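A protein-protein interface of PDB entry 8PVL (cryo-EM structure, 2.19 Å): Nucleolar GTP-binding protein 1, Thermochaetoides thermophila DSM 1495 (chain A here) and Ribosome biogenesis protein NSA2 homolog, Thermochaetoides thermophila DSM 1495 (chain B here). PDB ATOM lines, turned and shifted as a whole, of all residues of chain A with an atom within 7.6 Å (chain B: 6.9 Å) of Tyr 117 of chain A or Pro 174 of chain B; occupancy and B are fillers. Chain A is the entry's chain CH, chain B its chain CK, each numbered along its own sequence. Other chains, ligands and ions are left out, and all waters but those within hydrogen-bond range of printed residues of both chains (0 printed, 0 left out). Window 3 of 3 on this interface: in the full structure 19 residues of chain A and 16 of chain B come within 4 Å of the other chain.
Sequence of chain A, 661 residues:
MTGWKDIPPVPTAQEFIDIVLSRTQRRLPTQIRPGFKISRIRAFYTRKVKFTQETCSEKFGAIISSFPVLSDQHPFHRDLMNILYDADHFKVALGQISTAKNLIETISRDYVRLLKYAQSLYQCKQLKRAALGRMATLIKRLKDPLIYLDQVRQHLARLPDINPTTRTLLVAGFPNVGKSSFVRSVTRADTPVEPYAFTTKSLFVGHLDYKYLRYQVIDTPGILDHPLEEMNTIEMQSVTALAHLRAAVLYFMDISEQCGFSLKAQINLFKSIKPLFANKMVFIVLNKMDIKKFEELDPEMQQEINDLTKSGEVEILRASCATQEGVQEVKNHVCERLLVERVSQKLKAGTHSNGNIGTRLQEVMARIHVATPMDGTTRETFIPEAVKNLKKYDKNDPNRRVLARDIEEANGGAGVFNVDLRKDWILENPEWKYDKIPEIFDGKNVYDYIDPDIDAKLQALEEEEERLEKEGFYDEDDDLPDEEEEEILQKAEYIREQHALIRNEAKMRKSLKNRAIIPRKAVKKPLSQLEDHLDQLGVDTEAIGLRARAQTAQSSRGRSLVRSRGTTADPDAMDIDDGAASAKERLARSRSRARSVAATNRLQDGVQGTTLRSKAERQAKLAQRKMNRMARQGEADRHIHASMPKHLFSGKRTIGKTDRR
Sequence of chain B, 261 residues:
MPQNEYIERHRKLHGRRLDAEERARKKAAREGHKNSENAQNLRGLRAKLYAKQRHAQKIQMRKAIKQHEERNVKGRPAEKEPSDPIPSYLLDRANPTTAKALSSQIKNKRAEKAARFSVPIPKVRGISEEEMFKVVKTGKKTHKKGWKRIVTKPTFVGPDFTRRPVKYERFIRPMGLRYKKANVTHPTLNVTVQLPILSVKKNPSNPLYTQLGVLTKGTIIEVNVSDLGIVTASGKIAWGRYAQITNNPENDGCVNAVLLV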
ATOM      1  N   ILE A  38       9.334  -3.600  13.777  1.00  0.00           N
ATOM      2  CA  ILE A  38       8.057  -3.038  14.198  1.00  0.00           C
ATOM      3  C   ILE A  38       8.202  -2.279  15.513  1.00  0.00           C
ATOM      4  O   ILE A  38       7.516  -1.276  15.731  1.00  0.00           O
ATOM      5  CB  ILE A  38       6.987  -4.153  14.265  1.00  0.00           C
ATOM      6  CG1 ILE A  38       5.597  -3.569  14.533  1.00  0.00           C
ATOM      7  CG2 ILE A  38       7.351  -5.230  15.277  1.00  0.00           C
ATOM      8  CD1 ILE A  38       5.130  -2.611  13.465  1.00  0.00           C
ATOM      9  N   ARG A  42       7.144   1.574  15.952  1.00  0.00           N
ATOM     10  CA  ARG A  42       6.297   1.948  17.078  1.00  0.00           C
ATOM     11  C   ARG A  42       6.935   3.048  17.911  1.00  0.00           C
ATOM     12  O   ARG A  42       6.253   3.995  18.317  1.00  0.00           O
ATOM     13  CB  ARG A  42       6.020   0.731  17.958  1.00  0.00           C
ATOM     14  CG  ARG A  42       4.961  -0.221  17.449  1.00  0.00           C
ATOM     15  CD  ARG A  42       4.954  -1.482  18.295  1.00  0.00           C
ATOM     16  NE  ARG A  42       4.124  -2.537  17.729  1.00  0.00           N
ATOM     17  CZ  ARG A  42       4.154  -3.802  18.123  1.00  0.00           C
ATOM     18  NH1 ARG A  42       4.961  -4.207  19.088  1.00  0.00           N
ATOM     19  NH2 ARG A  42       3.347  -4.682  17.537  1.00  0.00           N
ATOM     20  N   TYR A 111      -3.649   7.004  22.472  1.00  0.00           N
ATOM     21  CA  TYR A 111      -3.026   6.599  21.217  1.00  0.00           C
ATOM     22  C   TYR A 111      -1.642   5.992  21.415  1.00  0.00           C
ATOM     23  O   TYR A 111      -1.231   5.151  20.612  1.00  0.00           O
ATOM     24  CB  TYR A 111      -2.991   7.774  20.246  1.00  0.00           C
ATOM     25  CG  TYR A 111      -4.307   7.913  19.523  1.00  0.00           C
ATOM     26  CD1 TYR A 111      -4.583   7.148  18.399  1.00  0.00           C
ATOM     27  CD2 TYR A 111      -5.290   8.772  19.990  1.00  0.00           C
ATOM     28  CE1 TYR A 111      -5.789   7.256  17.745  1.00  0.00           C
ATOM     29  CE2 TYR A 111      -6.501   8.886  19.343  1.00  0.00           C
ATOM     30  CZ  TYR A 111      -6.745   8.126  18.221  1.00  0.00           C
ATOM     31  OH  TYR A 111      -7.950   8.238  17.573  1.00  0.00           O
ATOM     32  N   VAL A 112      -0.929   6.359  22.485  1.00  0.00           N
ATOM     33  CA  VAL A 112       0.302   5.649  22.830  1.00  0.00           C
ATOM     34  C   VAL A 112      -0.010   4.203  23.210  1.00  0.00           C
ATOM     35  O   VAL A 112       0.690   3.263  22.793  1.00  0.00           O
ATOM     36  CB  VAL A 112       1.046   6.402  23.951  1.00  0.00           C
ATOM     37  CG1 VAL A 112       2.010   5.493  24.694  1.00  0.00           C
ATOM     38  CG2 VAL A 112       1.787   7.596  23.375  1.00  0.00           C
ATOM     39  N   ARG A 113      -1.096   4.002  23.969  1.00  0.00           N
ATOM     40  CA  ARG A 113      -1.510   2.651  24.333  1.00  0.00           C
ATOM     41  C   ARG A 113      -1.887   1.826  23.106  1.00  0.00           C
ATOM     42  O   ARG A 113      -1.613   0.623  23.052  1.00  0.00           O
ATOM     43  CB  ARG A 113      -2.674   2.715  25.322  1.00  0.00           C
ATOM     44  CG  ARG A 113      -2.839   1.468  26.168  1.00  0.00           C
ATOM     45  CD  ARG A 113      -4.052   1.553  27.081  1.00  0.00           C
ATOM     46  NE  ARG A 113      -3.986   2.664  28.023  1.00  0.00           N
ATOM     47  CZ  ARG A 113      -4.752   3.744  27.957  1.00  0.00           C
ATOM     48  NH1 ARG A 113      -5.643   3.900  26.993  1.00  0.00           N
ATOM     49  NH2 ARG A 113      -4.618   4.691  28.880  1.00  0.00           N
ATOM     50  N   LEU A 114      -2.521   2.454  22.110  1.00  0.00           N
ATOM     51  CA  LEU A 114      -2.849   1.729  20.879  1.00  0.00           C
ATOM     52  C   LEU A 114      -1.604   1.435  20.042  1.00  0.00           C
ATOM     53  O   LEU A 114      -1.496   0.363  19.423  1.00  0.00           O
ATOM     54  CB  LEU A 114      -3.866   2.519  20.059  1.00  0.00           C
ATOM     55  CG  LEU A 114      -5.224   2.735  20.721  1.00  0.00           C
ATOM     56  CD1 LEU A 114      -6.078   3.645  19.867  1.00  0.00           C
ATOM     57  CD2 LEU A 114      -5.921   1.410  20.966  1.00  0.00           C
ATOM     58  N   LEU A 115      -0.660   2.379  19.999  1.00  0.00           N
ATOM     59  CA  LEU A 115       0.583   2.171  19.268  1.00  0.00           C
ATOM     60  C   LEU A 115       1.435   1.071  19.878  1.00  0.00           C
ATOM     61  O   LEU A 115       2.289   0.514  19.181  1.00  0.00           O
ATOM     62  CB  LEU A 115       1.384   3.469  19.204  1.00  0.00           C
ATOM     63  CG  LEU A 115       0.927   4.466  18.143  1.00  0.00           C
ATOM     64  CD1 LEU A 115       1.717   5.757  18.243  1.00  0.00           C
ATOM     65  CD2 LEU A 115       1.058   3.858  16.763  1.00  0.00           C
ATOM     66  N   LYS A 116       1.236   0.766  21.164  1.00  0.00           N
ATOM     67  CA  LYS A 116       1.864  -0.425  21.736  1.00  0.00           C
ATOM     68  C   LYS A 116       1.447  -1.703  21.011  1.00  0.00           C
ATOM     69  O   LYS A 116       2.237  -2.649  20.923  1.00  0.00           O
ATOM     70  CB  LYS A 116       1.525  -0.561  23.220  1.00  0.00           C
ATOM     71  CG  LYS A 116       2.193   0.439  24.138  1.00  0.00           C
ATOM     72  CD  LYS A 116       2.185  -0.058  25.580  1.00  0.00           C
ATOM     73  CE  LYS A 116       0.822  -0.608  25.985  1.00  0.00           C
ATOM     74  NZ  LYS A 116       0.864  -1.305  27.297  1.00  0.00           N
ATOM     75  N   TYR A 117       0.220  -1.755  20.487  1.00  0.00           N
ATOM     76  CA  TYR A 117      -0.301  -2.964  19.868  1.00  0.00           C
ATOM     77  C   TYR A 117      -0.395  -2.898  18.351  1.00  0.00           C
ATOM     78  O   TYR A 117      -0.749  -3.909  17.735  1.00  0.00           O
ATOM     79  CB  TYR A 117      -1.690  -3.296  20.431  1.00  0.00           C
ATOM     80  CG  TYR A 117      -1.708  -3.546  21.918  1.00  0.00           C
ATOM     81  CD1 TYR A 117      -1.164  -4.705  22.452  1.00  0.00           C
ATOM     82  CD2 TYR A 117      -2.269  -2.621  22.787  1.00  0.00           C
ATOM     83  CE1 TYR A 117      -1.179  -4.935  23.811  1.00  0.00           C
ATOM     84  CE2 TYR A 117      -2.290  -2.844  24.147  1.00  0.00           C
ATOM     85  CZ  TYR A 117      -1.743  -4.001  24.653  1.00  0.00           C
ATOM     86  OH  TYR A 117      -1.761  -4.228  26.009  1.00  0.00           O
ATOM     87  N   ALA A 118      -0.119  -1.746  17.739  1.00  0.00           N
ATOM     88  CA  ALA A 118      -0.177  -1.643  16.282  1.00  0.00           C
ATOM     89  C   ALA A 118       0.849  -2.564  15.617  1.00  0.00           C
ATOM     90  O   ALA A 118       1.942  -2.794  16.139  1.00  0.00           O
ATOM     91  CB  ALA A 118       0.049  -0.200  15.843  1.00  0.00           C
ATOM     92  N   GLN A 119       0.480  -3.100  14.450  1.00  0.00           N
ATOM     93  CA  GLN A 119       1.207  -4.204  13.835  1.00  0.00           C
ATOM     94  C   GLN A 119       1.900  -3.873  12.522  1.00  0.00           C
ATOM     95  O   GLN A 119       2.581  -4.744  11.972  1.00  0.00           O
ATOM     96  CB  GLN A 119       0.262  -5.391  13.601  1.00  0.00           C
ATOM     97  CG  GLN A 119      -0.154  -6.123  14.860  1.00  0.00           C
ATOM     98  CD  GLN A 119       1.011  -6.801  15.550  1.00  0.00           C
ATOM     99  OE1 GLN A 119       1.950  -7.257  14.900  1.00  0.00           O
ATOM    100  NE2 GLN A 119       0.957  -6.868  16.872  1.00  0.00           N
ATOM    101  N   SER A 120       1.755  -2.661  11.994  1.00  0.00           N
ATOM    102  CA  SER A 120       2.383  -2.324  10.725  1.00  0.00           C
ATOM    103  C   SER A 120       2.650  -0.828  10.676  1.00  0.00           C
ATOM    104  O   SER A 120       2.121  -0.053  11.478  1.00  0.00           O
ATOM    105  CB  SER A 120       1.521  -2.758   9.536  1.00  0.00           C
ATOM    106  OG  SER A 120       0.427  -1.879   9.346  1.00  0.00           O
ATOM    107  N   GLN A 123      -0.622   1.080   9.853  1.00  0.00           N
ATOM    108  CA  GLN A 123      -1.481   1.232  11.023  1.00  0.00           C
ATOM    109  C   GLN A 123      -0.905   2.240  12.013  1.00  0.00           C
ATOM    110  O   GLN A 123      -1.649   3.048  12.584  1.00  0.00           O
ATOM    111  CB  GLN A 123      -1.690  -0.120  11.701  1.00  0.00           C
ATOM    112  CG  GLN A 123      -2.727  -0.092  12.809  1.00  0.00           C
ATOM    113  CD  GLN A 123      -2.723  -1.348  13.651  1.00  0.00           C
ATOM    114  OE1 GLN A 123      -1.948  -2.270  13.410  1.00  0.00           O
ATOM    115  NE2 GLN A 123      -3.589  -1.386  14.654  1.00  0.00           N
ATOM    116  N   CYS A 124       0.415   2.209  12.218  1.00  0.00           N
ATOM    117  CA  CYS A 124       1.063   3.177  13.100  1.00  0.00           C
ATOM    118  C   CYS A 124       0.910   4.598  12.571  1.00  0.00           C
ATOM    119  O   CYS A 124       0.647   5.531  13.340  1.00  0.00           O
ATOM    120  CB  CYS A 124       2.544   2.828  13.260  1.00  0.00           C
ATOM    121  SG  CYS A 124       2.925   1.442  14.349  1.00  0.00           S
ATOM    122  N   LEU A 127      -2.704   5.737  13.123  1.00  0.00           N
ATOM    123  CA  LEU A 127      -2.949   6.065  14.526  1.00  0.00           C
ATOM    124  C   LEU A 127      -2.299   7.389  14.919  1.00  0.00           C
ATOM    125  O   LEU A 127      -2.907   8.195  15.639  1.00  0.00           O
ATOM    126  CB  LEU A 127      -2.449   4.935  15.425  1.00  0.00           C
ATOM    127  CG  LEU A 127      -3.321   3.682  15.498  1.00  0.00           C
ATOM    128  CD1 LEU A 127      -2.679   2.634  16.389  1.00  0.00           C
ATOM    129  CD2 LEU A 127      -4.715   4.027  15.994  1.00  0.00           C
ATOM    130  N   ILE B 150      -2.732 -13.548  20.225  1.00  0.00           N
ATOM    131  CA  ILE B 150      -3.209 -12.240  20.667  1.00  0.00           C
ATOM    132  C   ILE B 150      -4.036 -11.619  19.548  1.00  0.00           C
ATOM    133  O   ILE B 150      -3.655 -11.678  18.372  1.00  0.00           O
ATOM    134  CB  ILE B 150      -2.040 -11.329  21.094  1.00  0.00           C
ATOM    135  CG1 ILE B 150      -2.534  -9.932  21.477  1.00  0.00           C
ATOM    136  CG2 ILE B 150      -0.962 -11.249  20.024  1.00  0.00           C
ATOM    137  CD1 ILE B 150      -1.453  -9.034  22.028  1.00  0.00           C
ATOM    138  N   VAL B 151      -5.195 -11.070  19.902  1.00  0.00           N
ATOM    139  CA  VAL B 151      -6.057 -10.416  18.923  1.00  0.00           C
ATOM    140  C   VAL B 151      -5.538  -9.007  18.673  1.00  0.00           C
ATOM    141  O   VAL B 151      -5.373  -8.216  19.609  1.00  0.00           O
ATOM    142  CB  VAL B 151      -7.515 -10.398  19.405  1.00  0.00           C
ATOM    143  CG1 VAL B 151      -8.435  -9.941  18.287  1.00  0.00           C
ATOM    144  CG2 VAL B 151      -7.922 -11.771  19.908  1.00  0.00           C
ATOM    145  N   THR B 152      -5.274  -8.693  17.410  1.00  0.00           N
ATOM    146  CA  THR B 152      -4.658  -7.429  17.027  1.00  0.00           C
ATOM    147  C   THR B 152      -5.672  -6.333  16.730  1.00  0.00           C
ATOM    148  O   THR B 152      -5.275  -5.182  16.525  1.00  0.00           O
ATOM    149  CB  THR B 152      -3.757  -7.638  15.806  1.00  0.00           C
ATOM    150  OG1 THR B 152      -4.543  -8.107  14.705  1.00  0.00           O
ATOM    151  CG2 THR B 152      -2.674  -8.657  16.114  1.00  0.00           C
ATOM    152  N   LYS B 153      -6.955  -6.654  16.706  1.00  0.00           N
ATOM    153  CA  LYS B 153      -8.022  -5.715  16.413  1.00  0.00           C
ATOM    154  C   LYS B 153      -8.763  -5.343  17.694  1.00  0.00           C
ATOM    155  O   LYS B 153      -8.653  -6.045  18.704  1.00  0.00           O
ATOM    156  CB  LYS B 153      -8.992  -6.329  15.393  1.00  0.00           C
ATOM    157  CG  LYS B 153      -8.315  -6.884  14.153  1.00  0.00           C
ATOM    158  CD  LYS B 153      -7.801  -5.792  13.237  1.00  0.00           C
ATOM    159  CE  LYS B 153      -7.193  -6.388  11.979  1.00  0.00           C
ATOM    160  NZ  LYS B 153      -6.632  -5.357  11.068  1.00  0.00           N
ATOM    161  N   THR B 155     -11.709  -5.080  20.431  1.00  0.00           N
ATOM    162  CA  THR B 155     -12.673  -6.080  20.864  1.00  0.00           C
ATOM    163  C   THR B 155     -13.679  -5.478  21.836  1.00  0.00           C
ATOM    164  O   THR B 155     -13.474  -4.400  22.399  1.00  0.00           O
ATOM    165  CB  THR B 155     -12.002  -7.290  21.541  1.00  0.00           C
ATOM    166  OG1 THR B 155     -11.233  -6.850  22.667  1.00  0.00           O
ATOM    167  CG2 THR B 155     -11.110  -8.051  20.573  1.00  0.00           C
ATOM    168  N   VAL B 157     -15.782  -7.083  25.174  1.00  0.00           N
ATOM    169  CA  VAL B 157     -15.803  -8.260  26.039  1.00  0.00           C
ATOM    170  C   VAL B 157     -17.100  -8.409  26.823  1.00  0.00           C
ATOM    171  O   VAL B 157     -17.323  -9.471  27.424  1.00  0.00           O
ATOM    172  CB  VAL B 157     -14.605  -8.260  27.014  1.00  0.00           C
ATOM    173  CG1 VAL B 157     -13.309  -8.456  26.250  1.00  0.00           C
ATOM    174  CG2 VAL B 157     -14.569  -6.970  27.816  1.00  0.00           C
ATOM    175  N   GLU B 169      -5.397 -19.576  29.001  1.00  0.00           N
ATOM    176  CA  GLU B 169      -5.818 -18.418  28.217  1.00  0.00           C
ATOM    177  C   GLU B 169      -5.154 -18.513  26.847  1.00  0.00           C
ATOM    178  O   GLU B 169      -3.992 -18.135  26.682  1.00  0.00           O
ATOM    179  CB  GLU B 169      -5.457 -17.117  28.929  1.00  0.00           C
ATOM    180  CG  GLU B 169      -5.916 -15.862  28.207  1.00  0.00           C
ATOM    181  CD  GLU B 169      -5.143 -14.631  28.633  1.00  0.00           C
ATOM    182  OE1 GLU B 169      -4.184 -14.771  29.418  1.00  0.00           O
ATOM    183  OE2 GLU B 169      -5.491 -13.521  28.182  1.00  0.00           O
ATOM    184  N   ILE B 172      -5.736 -13.903  23.716  1.00  0.00           N
ATOM    185  CA  ILE B 172      -5.453 -12.728  24.523  1.00  0.00           C
ATOM    186  C   ILE B 172      -6.125 -11.536  23.864  1.00  0.00           C
ATOM    187  O   ILE B 172      -5.765 -11.145  22.748  1.00  0.00           O
ATOM    188  CB  ILE B 172      -3.941 -12.495  24.666  1.00  0.00           C
ATOM    189  CG1 ILE B 172      -3.276 -13.693  25.346  1.00  0.00           C
ATOM    190  CG2 ILE B 172      -3.671 -11.210  25.433  1.00  0.00           C
ATOM    191  CD1 ILE B 172      -1.785 -13.763  25.129  1.00  0.00           C
ATOM    192  N   ARG B 173      -7.103 -10.962  24.552  1.00  0.00           N
ATOM    193  CA  ARG B 173      -7.717  -9.710  24.126  1.00  0.00           C
ATOM    194  C   ARG B 173      -7.206  -8.623  25.055  1.00  0.00           C
ATOM    195  O   ARG B 173      -7.729  -8.469  26.169  1.00  0.00           O
ATOM    196  CB  ARG B 173      -9.244  -9.802  24.178  1.00  0.00           C
ATOM    197  CG  ARG B 173      -9.831 -10.680  23.092  1.00  0.00           C
ATOM    198  CD  ARG B 173     -11.325 -10.847  23.255  1.00  0.00           C
ATOM    199  NE  ARG B 173     -11.655 -11.797  24.309  1.00  0.00           N
ATOM    200  CZ  ARG B 173     -12.890 -12.096  24.686  1.00  0.00           C
ATOM    201  NH1 ARG B 173     -13.942 -11.535  24.114  1.00  0.00           N
ATOM    202  NH2 ARG B 173     -13.075 -12.982  25.658  1.00  0.00           N
ATOM    203  N   PRO B 174      -6.177  -7.871  24.662  1.00  0.00           N
ATOM    204  CA  PRO B 174      -5.516  -6.962  25.604  1.00  0.00           C
ATOM    205  C   PRO B 174      -6.419  -5.829  26.064  1.00  0.00           C
ATOM    206  O   PRO B 174      -7.333  -5.401  25.355  1.00  0.00           O
ATOM    207  CB  PRO B 174      -4.317  -6.429  24.810  1.00  0.00           C
ATOM    208  CG  PRO B 174      -4.605  -6.737  23.393  1.00  0.00           C
ATOM    209  CD  PRO B 174      -5.472  -7.944  23.372  1.00  0.00           C
ATOM    210  N   MET B 175      -6.145  -5.361  27.286  1.00  0.00           N
ATOM    211  CA  MET B 175      -7.010  -4.391  27.952  1.00  0.00           C
ATOM    212  C   MET B 175      -7.072  -3.076  27.188  1.00  0.00           C
ATOM    213  O   MET B 175      -8.142  -2.466  27.076  1.00  0.00           O
ATOM    214  CB  MET B 175      -6.514  -4.151  29.376  1.00  0.00           C
ATOM    215  CG  MET B 175      -7.068  -5.113  30.406  1.00  0.00           C
ATOM    216  SD  MET B 175      -6.656  -4.605  32.084  1.00  0.00           S
ATOM    217  CE  MET B 175      -5.199  -5.593  32.389  1.00  0.00           C
ATOM    218  N   GLY B 176      -5.942  -2.631  26.642  1.00  0.00           N
ATOM    219  CA  GLY B 176      -5.892  -1.373  25.920  1.00  0.00           C
ATOM    220  C   GLY B 176      -6.572  -1.385  24.569  1.00  0.00           C
ATOM    221  O   GLY B 176      -6.671  -0.326  23.941  1.00  0.00           O
ATOM    222  N   LEU B 177      -7.037  -2.544  24.108  1.00  0.00           N
ATOM    223  CA  LEU B 177      -7.765  -2.647  22.853  1.00  0.00           C
ATOM    224  C   LEU B 177      -9.256  -2.894  23.056  1.00  0.00           C
ATOM    225  O   LEU B 177      -9.971  -3.125  22.078  1.00  0.00           O
ATOM    226  CB  LEU B 177      -7.160  -3.753  21.986  1.00  0.00           C
ATOM    227  CG  LEU B 177      -5.905  -3.380  21.197  1.00  0.00           C
ATOM    228  CD1 LEU B 177      -5.341  -4.585  20.462  1.00  0.00           C
ATOM    229  CD2 LEU B 177      -6.207  -2.259  20.227  1.00  0.00           C
ATOM    230  N   ARG B 178      -9.744  -2.846  24.293  1.00  0.00           N
ATOM    231  CA  ARG B 178     -11.146  -3.116  24.584  1.00  0.00           C
ATOM    232  C   ARG B 178     -11.954  -1.824  24.543  1.00  0.00           C
ATOM    233  O   ARG B 178     -11.562  -0.819  25.141  1.00  0.00           O
ATOM    234  CB  ARG B 178     -11.300  -3.787  25.949  1.00  0.00           C
ATOM    235  CG  ARG B 178     -10.680  -5.167  26.052  1.00  0.00           C
ATOM    236  CD  ARG B 178     -10.779  -5.704  27.469  1.00  0.00           C
ATOM    237  NE  ARG B 178      -9.836  -6.784  27.723  1.00  0.00           N
ATOM    238  CZ  ARG B 178      -9.560  -7.271  28.925  1.00  0.00           C
ATOM    239  NH1 ARG B 178     -10.156  -6.809  30.011  1.00  0.00           N
ATOM    240  NH2 ARG B 178      -8.665  -8.246  29.041  1.00  0.00           N
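NH2 of Arg 42 of chain A lies close to NE2 of Gln 119 of chain A, at 3.3 Å. The side-chain amide oxygen (OE1) of Gln 123 of chain A sits at hydrogen-bond distance from the backbone NH (N) of Gln 119 of chain A (2.8 Å). N of Thr 155 of chain B lies within hydrogen-bond range of O of Leu 177 of chain B.
Of the 15 printed residues of chain A, 4 touch a printed residue of chain B. Among the printed residues, 6 pairs touch across the chains.
Among the printed residues, merely in contact across the chains: Arg 113 of chain A with Gly 176 of chain B (3.6 Å), Leu 114 of chain A with Gly 176 of chain B (3.5 Å), Leu 114 of chain A with Leu 177 of chain B (3.8 Å), Tyr 117 of chain A with Pro 174 of chain B (3.5 Å), Tyr 117 of chain A with Leu 177 of chain B (3.9 Å) and Gln 119 of chain A with Thr 152 of chain B (3.8 Å).
Of the printed residues of chain B, Arg 113 of chain A touches Gly 176 (3.6 Å). Tyr 117 of chain A touches just these residues of chain B: Pro 174 (3.5 Å) and Leu 177 (3.9 Å). Printed residues of chain B within 4 Å of Gln 119 of chain A: Thr 152 (3.8 Å). The nearest printed residue of chain A that does not touch Pro 174 of chain B is Lys 116 of chain A (7.7 Å).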
